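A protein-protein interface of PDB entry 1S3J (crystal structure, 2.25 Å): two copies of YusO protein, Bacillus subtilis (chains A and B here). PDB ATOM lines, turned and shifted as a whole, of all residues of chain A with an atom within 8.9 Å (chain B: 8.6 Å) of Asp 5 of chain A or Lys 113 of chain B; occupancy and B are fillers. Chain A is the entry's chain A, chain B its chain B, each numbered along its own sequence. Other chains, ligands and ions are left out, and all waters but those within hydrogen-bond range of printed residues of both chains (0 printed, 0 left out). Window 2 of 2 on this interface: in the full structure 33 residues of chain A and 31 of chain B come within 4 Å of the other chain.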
ATOM      1  N   SER A   3     -14.284  -0.945  -3.922  1.00  0.00           N
ATOM      2  CA  SER A   3     -14.949  -0.580  -5.202  1.00  0.00           C
ATOM      3  C   SER A   3     -14.339  -1.376  -6.365  1.00  0.00           C
ATOM      4  O   SER A   3     -13.396  -0.918  -7.023  1.00  0.00           O
ATOM      5  CB  SER A   3     -14.827   0.930  -5.451  1.00  0.00           C
ATOM      6  OG  SER A   3     -15.321   1.275  -6.738  1.00  0.00           O
ATOM      7  N   ALA A   4     -14.903  -2.558  -6.612  1.00  0.00           N
ATOM      8  CA  ALA A   4     -14.337  -3.548  -7.536  1.00  0.00           C
ATOM      9  C   ALA A   4     -13.847  -2.995  -8.881  1.00  0.00           C
ATOM     10  O   ALA A   4     -12.854  -3.468  -9.394  1.00  0.00           O
ATOM     11  CB  ALA A   4     -15.344  -4.666  -7.778  1.00  0.00           C
ATOM     12  N   ASP A   5     -14.533  -2.010  -9.448  1.00  0.00           N
ATOM     13  CA  ASP A   5     -14.205  -1.554 -10.791  1.00  0.00           C
ATOM     14  C   ASP A   5     -12.923  -0.707 -10.845  1.00  0.00           C
ATOM     15  O   ASP A   5     -12.104  -0.866 -11.761  1.00  0.00           O
ATOM     16  CB  ASP A   5     -15.392  -0.818 -11.427  1.00  0.00           C
ATOM     17  CG  ASP A   5     -16.405  -1.773 -12.057  1.00  0.00           C
ATOM     18  OD1 ASP A   5     -16.628  -2.887 -11.507  1.00  0.00           O
ATOM     19  OD2 ASP A   5     -17.020  -1.491 -13.106  1.00  0.00           O
ATOM     20  N   GLN A   6     -12.741   0.181  -9.872  1.00  0.00           N
ATOM     21  CA  GLN A   6     -11.463   0.874  -9.765  1.00  0.00           C
ATOM     22  C   GLN A   6     -10.349  -0.133  -9.490  1.00  0.00           C
ATOM     23  O   GLN A   6      -9.274  -0.024 -10.069  1.00  0.00           O
ATOM     24  CB  GLN A   6     -11.462   1.958  -8.688  1.00  0.00           C
ATOM     25  CG  GLN A   6     -10.143   2.755  -8.659  1.00  0.00           C
ATOM     26  CD  GLN A   6      -9.830   3.385 -10.012  1.00  0.00           C
ATOM     27  OE1 GLN A   6     -10.663   4.112 -10.564  1.00  0.00           O
ATOM     28  NE2 GLN A   6      -8.650   3.087 -10.560  1.00  0.00           N
ATOM     29  N   LEU A   7     -10.625  -1.112  -8.626  1.00  0.00           N
ATOM     30  CA  LEU A   7      -9.644  -2.132  -8.246  1.00  0.00           C
ATOM     31  C   LEU A   7      -9.186  -2.969  -9.451  1.00  0.00           C
ATOM     32  O   LEU A   7      -8.012  -3.317  -9.566  1.00  0.00           O
ATOM     33  CB  LEU A   7     -10.201  -3.043  -7.139  1.00  0.00           C
ATOM     34  CG  LEU A   7      -9.201  -4.016  -6.488  1.00  0.00           C
ATOM     35  CD1 LEU A   7      -8.044  -3.266  -5.796  1.00  0.00           C
ATOM     36  CD2 LEU A   7      -9.904  -4.929  -5.508  1.00  0.00           C
ATOM     37  N   MET A   8     -10.116  -3.266 -10.350  1.00  0.00           N
ATOM     38  CA  MET A   8      -9.798  -3.968 -11.594  1.00  0.00           C
ATOM     39  C   MET A   8      -8.977  -3.093 -12.538  1.00  0.00           C
ATOM     40  O   MET A   8      -8.098  -3.585 -13.233  1.00  0.00           O
ATOM     41  CB  MET A   8     -11.077  -4.412 -12.296  1.00  0.00           C
ATOM     42  CG  MET A   8     -11.694  -5.652 -11.665  1.00  0.00           C
ATOM     43  SD  MET A   8     -13.188  -6.384 -12.694  1.00  0.00           S
ATOM     44  CE  MET A   8     -14.662  -5.664 -11.654  1.00  0.00           C
ATOM     45  N   SER A   9      -9.265  -1.796 -12.558  1.00  0.00           N
ATOM     46  CA  SER A   9      -8.538  -0.870 -13.429  1.00  0.00           C
ATOM     47  C   SER A   9      -7.103  -0.652 -12.950  1.00  0.00           C
ATOM     48  O   SER A   9      -6.188  -0.533 -13.778  1.00  0.00           O
ATOM     49  CB  SER A   9      -9.267   0.469 -13.547  1.00  0.00           C
ATOM     50  OG  SER A   9     -10.362   0.342 -14.431  1.00  0.00           O
ATOM     51  N   ASP A  10      -6.921  -0.605 -11.626  1.00  0.00           N
ATOM     52  CA  ASP A  10      -5.597  -0.492 -11.007  1.00  0.00           C
ATOM     53  C   ASP A  10      -4.759  -1.719 -11.388  1.00  0.00           C
ATOM     54  O   ASP A  10      -3.653  -1.585 -11.876  1.00  0.00           O
ATOM     55  CB  ASP A  10      -5.682  -0.423  -9.474  1.00  0.00           C
ATOM     56  CG  ASP A  10      -6.454   0.795  -8.951  1.00  0.00           C
ATOM     57  OD1 ASP A  10      -6.465   1.877  -9.591  1.00  0.00           O
ATOM     58  OD2 ASP A  10      -7.079   0.751  -7.874  1.00  0.00           O
ATOM     59  N   ILE A  11      -5.318  -2.904 -11.170  1.00  0.00           N
ATOM     60  CA  ILE A  11      -4.626  -4.148 -11.441  1.00  0.00           C
ATOM     61  C   ILE A  11      -4.298  -4.298 -12.902  1.00  0.00           C
ATOM     62  O   ILE A  11      -3.192  -4.703 -13.241  1.00  0.00           O
ATOM     63  CB  ILE A  11      -5.456  -5.353 -10.982  1.00  0.00           C
ATOM     64  CG1 ILE A  11      -5.429  -5.439  -9.468  1.00  0.00           C
ATOM     65  CG2 ILE A  11      -4.909  -6.646 -11.590  1.00  0.00           C
ATOM     66  CD1 ILE A  11      -6.263  -6.571  -8.881  1.00  0.00           C
ATOM     67  N   GLN A  12      -5.267  -4.012 -13.760  1.00  0.00           N
ATOM     68  CA  GLN A  12      -5.084  -4.122 -15.191  1.00  0.00           C
ATOM     69  C   GLN A  12      -3.902  -3.251 -15.587  1.00  0.00           C
ATOM     70  O   GLN A  12      -3.018  -3.684 -16.318  1.00  0.00           O
ATOM     71  CB  GLN A  12      -6.364  -3.692 -15.937  1.00  0.00           C
ATOM     72  CG  GLN A  12      -6.332  -3.924 -17.450  1.00  0.00           C
ATOM     73  CD  GLN A  12      -5.572  -2.857 -18.215  1.00  0.00           C
ATOM     74  OE1 GLN A  12      -5.537  -1.694 -17.795  1.00  0.00           O
ATOM     75  NE2 GLN A  12      -4.971  -3.243 -19.352  1.00  0.00           N
ATOM     76  N   MET B  26      -7.422 -14.550 -24.247  1.00  0.00           N
ATOM     77  CA  MET B  26      -7.595 -13.151 -24.643  1.00  0.00           C
ATOM     78  C   MET B  26      -7.532 -13.008 -26.160  1.00  0.00           C
ATOM     79  O   MET B  26      -8.279 -12.238 -26.730  1.00  0.00           O
ATOM     80  CB  MET B  26      -6.526 -12.253 -24.035  1.00  0.00           C
ATOM     81  CG  MET B  26      -6.256 -12.495 -22.583  1.00  0.00           C
ATOM     82  SD  MET B  26      -6.369 -10.887 -21.575  1.00  0.00           S
ATOM     83  CE  MET B  26      -8.207 -10.878 -21.358  1.00  0.00           C
ATOM     84  N   SER B  29     -10.820 -14.378 -27.663  1.00  0.00           N
ATOM     85  CA  SER B  29     -11.865 -13.378 -27.471  1.00  0.00           C
ATOM     86  C   SER B  29     -11.797 -12.259 -28.534  1.00  0.00           C
ATOM     87  O   SER B  29     -12.834 -11.821 -29.027  1.00  0.00           O
ATOM     88  CB  SER B  29     -11.769 -12.760 -26.082  1.00  0.00           C
ATOM     89  OG  SER B  29     -12.835 -11.841 -25.872  1.00  0.00           O
ATOM     90  N   GLU B 106     -15.560  -1.196 -27.245  1.00  0.00           N
ATOM     91  CA  GLU B 106     -16.024  -1.419 -25.884  1.00  0.00           C
ATOM     92  C   GLU B 106     -16.290  -2.907 -25.647  1.00  0.00           C
ATOM     93  O   GLU B 106     -15.999  -3.416 -24.569  1.00  0.00           O
ATOM     94  CB  GLU B 106     -17.273  -0.587 -25.557  1.00  0.00           C
ATOM     95  CG  GLU B 106     -17.034   0.913 -25.485  1.00  0.00           C
ATOM     96  CD  GLU B 106     -15.975   1.323 -24.463  1.00  0.00           C
ATOM     97  OE1 GLU B 106     -15.756   0.568 -23.482  1.00  0.00           O
ATOM     98  OE2 GLU B 106     -15.362   2.406 -24.637  1.00  0.00           O
ATOM     99  N   GLU B 107     -16.786  -3.597 -26.668  1.00  0.00           N
ATOM    100  CA  GLU B 107     -17.007  -5.037 -26.595  1.00  0.00           C
ATOM    101  C   GLU B 107     -15.712  -5.799 -26.344  1.00  0.00           C
ATOM    102  O   GLU B 107     -15.734  -6.778 -25.612  1.00  0.00           O
ATOM    103  CB  GLU B 107     -17.635  -5.592 -27.874  1.00  0.00           C
ATOM    104  CG  GLU B 107     -19.119  -5.340 -28.029  1.00  0.00           C
ATOM    105  CD  GLU B 107     -19.662  -5.835 -29.364  1.00  0.00           C
ATOM    106  OE1 GLU B 107     -18.876  -6.157 -30.288  1.00  0.00           O
ATOM    107  OE2 GLU B 107     -20.893  -5.898 -29.495  1.00  0.00           O
ATOM    108  N   VAL B 108     -14.606  -5.360 -26.970  1.00  0.00           N
ATOM    109  CA  VAL B 108     -13.329  -6.031 -26.805  1.00  0.00           C
ATOM    110  C   VAL B 108     -12.831  -5.786 -25.375  1.00  0.00           C
ATOM    111  O   VAL B 108     -12.346  -6.721 -24.737  1.00  0.00           O
ATOM    112  CB  VAL B 108     -12.250  -5.571 -27.823  1.00  0.00           C
ATOM    113  CG1 VAL B 108     -10.856  -6.072 -27.420  1.00  0.00           C
ATOM    114  CG2 VAL B 108     -12.605  -6.013 -29.242  1.00  0.00           C
ATOM    115  N   LEU B 109     -12.954  -4.548 -24.892  1.00  0.00           N
ATOM    116  CA  LEU B 109     -12.537  -4.197 -23.534  1.00  0.00           C
ATOM    117  C   LEU B 109     -13.332  -4.952 -22.482  1.00  0.00           C
ATOM    118  O   LEU B 109     -12.789  -5.312 -21.449  1.00  0.00           O
ATOM    119  CB  LEU B 109     -12.679  -2.694 -23.272  1.00  0.00           C
ATOM    120  CG  LEU B 109     -11.390  -1.851 -23.259  1.00  0.00           C
ATOM    121  CD1 LEU B 109     -10.421  -2.270 -24.346  1.00  0.00           C
ATOM    122  CD2 LEU B 109     -11.760  -0.383 -23.403  1.00  0.00           C
ATOM    123  N   ALA B 110     -14.623  -5.168 -22.742  1.00  0.00           N
ATOM    124  CA  ALA B 110     -15.476  -5.867 -21.806  1.00  0.00           C
ATOM    125  C   ALA B 110     -15.139  -7.347 -21.827  1.00  0.00           C
ATOM    126  O   ALA B 110     -15.245  -8.011 -20.823  1.00  0.00           O
ATOM    127  CB  ALA B 110     -16.934  -5.642 -22.129  1.00  0.00           C
ATOM    128  N   GLY B 111     -14.709  -7.862 -22.976  1.00  0.00           N
ATOM    129  CA  GLY B 111     -14.356  -9.265 -23.081  1.00  0.00           C
ATOM    130  C   GLY B 111     -13.104  -9.566 -22.265  1.00  0.00           C
ATOM    131  O   GLY B 111     -12.988 -10.645 -21.662  1.00  0.00           O
ATOM    132  N   ARG B 112     -12.168  -8.617 -22.270  1.00  0.00           N
ATOM    133  CA  ARG B 112     -10.905  -8.741 -21.553  1.00  0.00           C
ATOM    134  C   ARG B 112     -11.120  -8.595 -20.051  1.00  0.00           C
ATOM    135  O   ARG B 112     -10.518  -9.300 -19.266  1.00  0.00           O
ATOM    136  CB  ARG B 112      -9.916  -7.650 -21.967  1.00  0.00           C
ATOM    137  CG  ARG B 112      -9.411  -7.695 -23.373  1.00  0.00           C
ATOM    138  CD  ARG B 112      -8.433  -6.538 -23.686  1.00  0.00           C
ATOM    139  NE  ARG B 112      -7.053  -6.982 -23.585  1.00  0.00           N
ATOM    140  CZ  ARG B 112      -6.473  -7.807 -24.454  1.00  0.00           C
ATOM    141  NH1 ARG B 112      -7.148  -8.267 -25.501  1.00  0.00           N
ATOM    142  NH2 ARG B 112      -5.212  -8.194 -24.276  1.00  0.00           N
ATOM    143  N   LYS B 113     -11.956  -7.646 -19.665  1.00  0.00           N
ATOM    144  CA  LYS B 113     -12.239  -7.408 -18.268  1.00  0.00           C
ATOM    145  C   LYS B 113     -12.957  -8.621 -17.651  1.00  0.00           C
ATOM    146  O   LYS B 113     -12.705  -8.970 -16.493  1.00  0.00           O
ATOM    147  CB  LYS B 113     -13.089  -6.153 -18.126  1.00  0.00           C
ATOM    148  CG  LYS B 113     -13.654  -5.906 -16.728  1.00  0.00           C
ATOM    149  CD  LYS B 113     -14.340  -4.547 -16.641  1.00  0.00           C
ATOM    150  CE  LYS B 113     -15.038  -4.383 -15.297  1.00  0.00           C
ATOM    151  NZ  LYS B 113     -16.056  -3.296 -15.303  1.00  0.00           N
ATOM    152  N   ALA B 114     -13.851  -9.251 -18.410  1.00  0.00           N
ATOM    153  CA  ALA B 114     -14.562 -10.421 -17.906  1.00  0.00           C
ATOM    154  C   ALA B 114     -13.597 -11.614 -17.713  1.00  0.00           C
ATOM    155  O   ALA B 114     -13.772 -12.393 -16.794  1.00  0.00           O
ATOM    156  CB  ALA B 114     -15.762 -10.817 -18.840  1.00  0.00           C
ATOM    157  N   ILE B 115     -12.594 -11.747 -18.582  1.00  0.00           N
ATOM    158  CA  ILE B 115     -11.625 -12.833 -18.453  1.00  0.00           C
ATOM    159  C   ILE B 115     -10.815 -12.628 -17.186  1.00  0.00           C
ATOM    160  O   ILE B 115     -10.554 -13.583 -16.480  1.00  0.00           O
ATOM    161  CB  ILE B 115     -10.719 -12.975 -19.703  1.00  0.00           C
ATOM    162  CG1 ILE B 115     -11.516 -13.598 -20.833  1.00  0.00           C
ATOM    163  CG2 ILE B 115      -9.491 -13.858 -19.418  1.00  0.00           C
ATOM    164  CD1 ILE B 115     -10.876 -13.443 -22.197  1.00  0.00           C
ATOM    165  N   MET B 116     -10.479 -11.383 -16.864  1.00  0.00           N
ATOM    166  CA  MET B 116      -9.739 -11.101 -15.644  1.00  0.00           C
ATOM    167  C   MET B 116     -10.616 -11.065 -14.382  1.00  0.00           C
ATOM    168  O   MET B 116     -10.137 -11.424 -13.305  1.00  0.00           O
ATOM    169  CB  MET B 116      -8.919  -9.821 -15.782  1.00  0.00           C
ATOM    170  CG  MET B 116      -7.600 -10.046 -16.509  1.00  0.00           C
ATOM    171  SD  MET B 116      -6.219 -11.188 -15.598  1.00  0.00           S
ATOM    172  CE  MET B 116      -5.113 -11.333 -17.145  1.00  0.00           C
ATOM    173  N   ALA B 117     -11.880 -10.657 -14.491  1.00  0.00           N
ATOM    174  CA  ALA B 117     -12.797 -10.762 -13.344  1.00  0.00           C
ATOM    175  C   ALA B 117     -12.989 -12.222 -12.911  1.00  0.00           C
ATOM    176  O   ALA B 117     -13.202 -12.490 -11.733  1.00  0.00           O
ATOM    177  CB  ALA B 117     -14.140 -10.141 -13.635  1.00  0.00           C
ATOM    178  N   ARG B 118     -12.901 -13.145 -13.862  1.00  0.00           N
ATOM    179  CA  ARG B 118     -13.026 -14.563 -13.575  1.00  0.00           C
ATOM    180  C   ARG B 118     -11.809 -15.165 -12.867  1.00  0.00           C
ATOM    181  O   ARG B 118     -11.960 -15.914 -11.909  1.00  0.00           O
ATOM    182  CB  ARG B 118     -13.313 -15.363 -14.848  1.00  0.00           C
ATOM    183  CG  ARG B 118     -13.897 -16.718 -14.527  1.00  0.00           C
ATOM    184  CD  ARG B 118     -14.231 -17.567 -15.712  1.00  0.00           C
ATOM    185  NE  ARG B 118     -13.056 -18.259 -16.228  1.00  0.00           N
ATOM    186  CZ  ARG B 118     -12.337 -17.875 -17.285  1.00  0.00           C
ATOM    187  NH1 ARG B 118     -12.655 -16.774 -17.981  1.00  0.00           N
ATOM    188  NH2 ARG B 118     -11.290 -18.612 -17.657  1.00  0.00           N
ATOM    189  N   TYR B 119     -10.605 -14.868 -13.350  1.00  0.00           N
ATOM    190  CA  TYR B 119      -9.399 -15.370 -12.695  1.00  0.00           C
ATOM    191  C   TYR B 119      -9.275 -14.831 -11.274  1.00  0.00           C
ATOM    192  O   TYR B 119      -8.767 -15.519 -10.403  1.00  0.00           O
ATOM    193  CB  TYR B 119      -8.138 -15.056 -13.511  1.00  0.00           C
ATOM    194  CG  TYR B 119      -7.925 -16.014 -14.645  1.00  0.00           C
ATOM    195  CD1 TYR B 119      -8.492 -15.781 -15.877  1.00  0.00           C
ATOM    196  CD2 TYR B 119      -7.168 -17.170 -14.473  1.00  0.00           C
ATOM    197  CE1 TYR B 119      -8.318 -16.664 -16.920  1.00  0.00           C
ATOM    198  CE2 TYR B 119      -6.973 -18.062 -15.512  1.00  0.00           C
ATOM    199  CZ  TYR B 119      -7.552 -17.814 -16.730  1.00  0.00           C
ATOM    200  OH  TYR B 119      -7.360 -18.693 -17.780  1.00  0.00           O
ATOM    201  N   LEU B 120      -9.786 -13.636 -11.032  1.00  0.00           N
ATOM    202  CA  LEU B 120      -9.683 -12.988  -9.736  1.00  0.00           C
ATOM    203  C   LEU B 120     -10.831 -13.339  -8.788  1.00  0.00           C
ATOM    204  O   LEU B 120     -10.687 -13.212  -7.569  1.00  0.00           O
ATOM    205  CB  LEU B 120      -9.611 -11.468  -9.924  1.00  0.00           C
ATOM    206  CG  LEU B 120      -8.439 -10.835 -10.718  1.00  0.00           C
ATOM    207  CD1 LEU B 120      -7.931  -9.548 -10.073  1.00  0.00           C
ATOM    208  CD2 LEU B 120      -7.247 -11.765 -10.959  1.00  0.00           C
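The side-chain carboxylate (OD2) of Asp 5 of chain A is in salt-bridge range of the side-chain amino group (NZ) of Lys 113 of chain B, 3.0 Å away.
O of Asp 5 of chain A sits at hydrogen-bond distance from OG of Ser 9 of chain A (3.4 Å).
Asp 5 of chain A touches just one residue of chain B: Lys 113.
Lys 113 of chain B touches just these residues of chain A: Asp 5 (3.0 Å) and Met 8 (3.8 Å).
No residue of chain A comes within 4 Å of Ala 114 of chain B.
Of the printed residues of chain A, Leu 120 of chain B touches Ile 11 (3.6 Å).
Of the printed residues of chain B, Met 8 of chain A touches Lys 113 (3.8 Å) and Ala 117 (3.99 Å).
Of the printed residues of chain A, Ala 117 of chain B touches Met 8 (3.99 Å).
Of the printed residues of chain B, Ile 11 of chain A touches Leu 120 (3.6 Å).
The nearest residue of chain B that does not touch Asp 5 of chain A is Ala 117 of chain B (8.0 Å).
The nearest residue of chain A that does not touch Lys 113 of chain B is Ala 4 of chain A (6.4 Å).
The nearest printed residue of chain A that does not touch Ala 117 of chain B is Asp 5 of chain A (8.0 Å).
Among the printed residues, pairs that only touch across the chains: Ile 11 of chain A with Leu 120 of chain B, Met 8 of chain A with Lys 113 of chain B and Met 8 of chain A with Ala 117 of chain B.
No position is printed for both chains.
Of the 4 pairs that touch across the chains among the printed residues, none has its exchanged pair printed and touching as well.
Hydrophobic or aromatic side chains of chain B that line the printed part of chain A: Ala 117 and Leu 120.
Along chain B the printed residues that touch a printed residue of chain A span positions 113 to 120.
Of the 10 printed residues of chain A, 3 touch a printed residue of chain B.
Among the printed residues, Asp or Glu carboxylates within 4 Å of a Lys or Arg side-chain nitrogen of the other chain: Asp 5 of chain A with Lys 113 of chain B.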
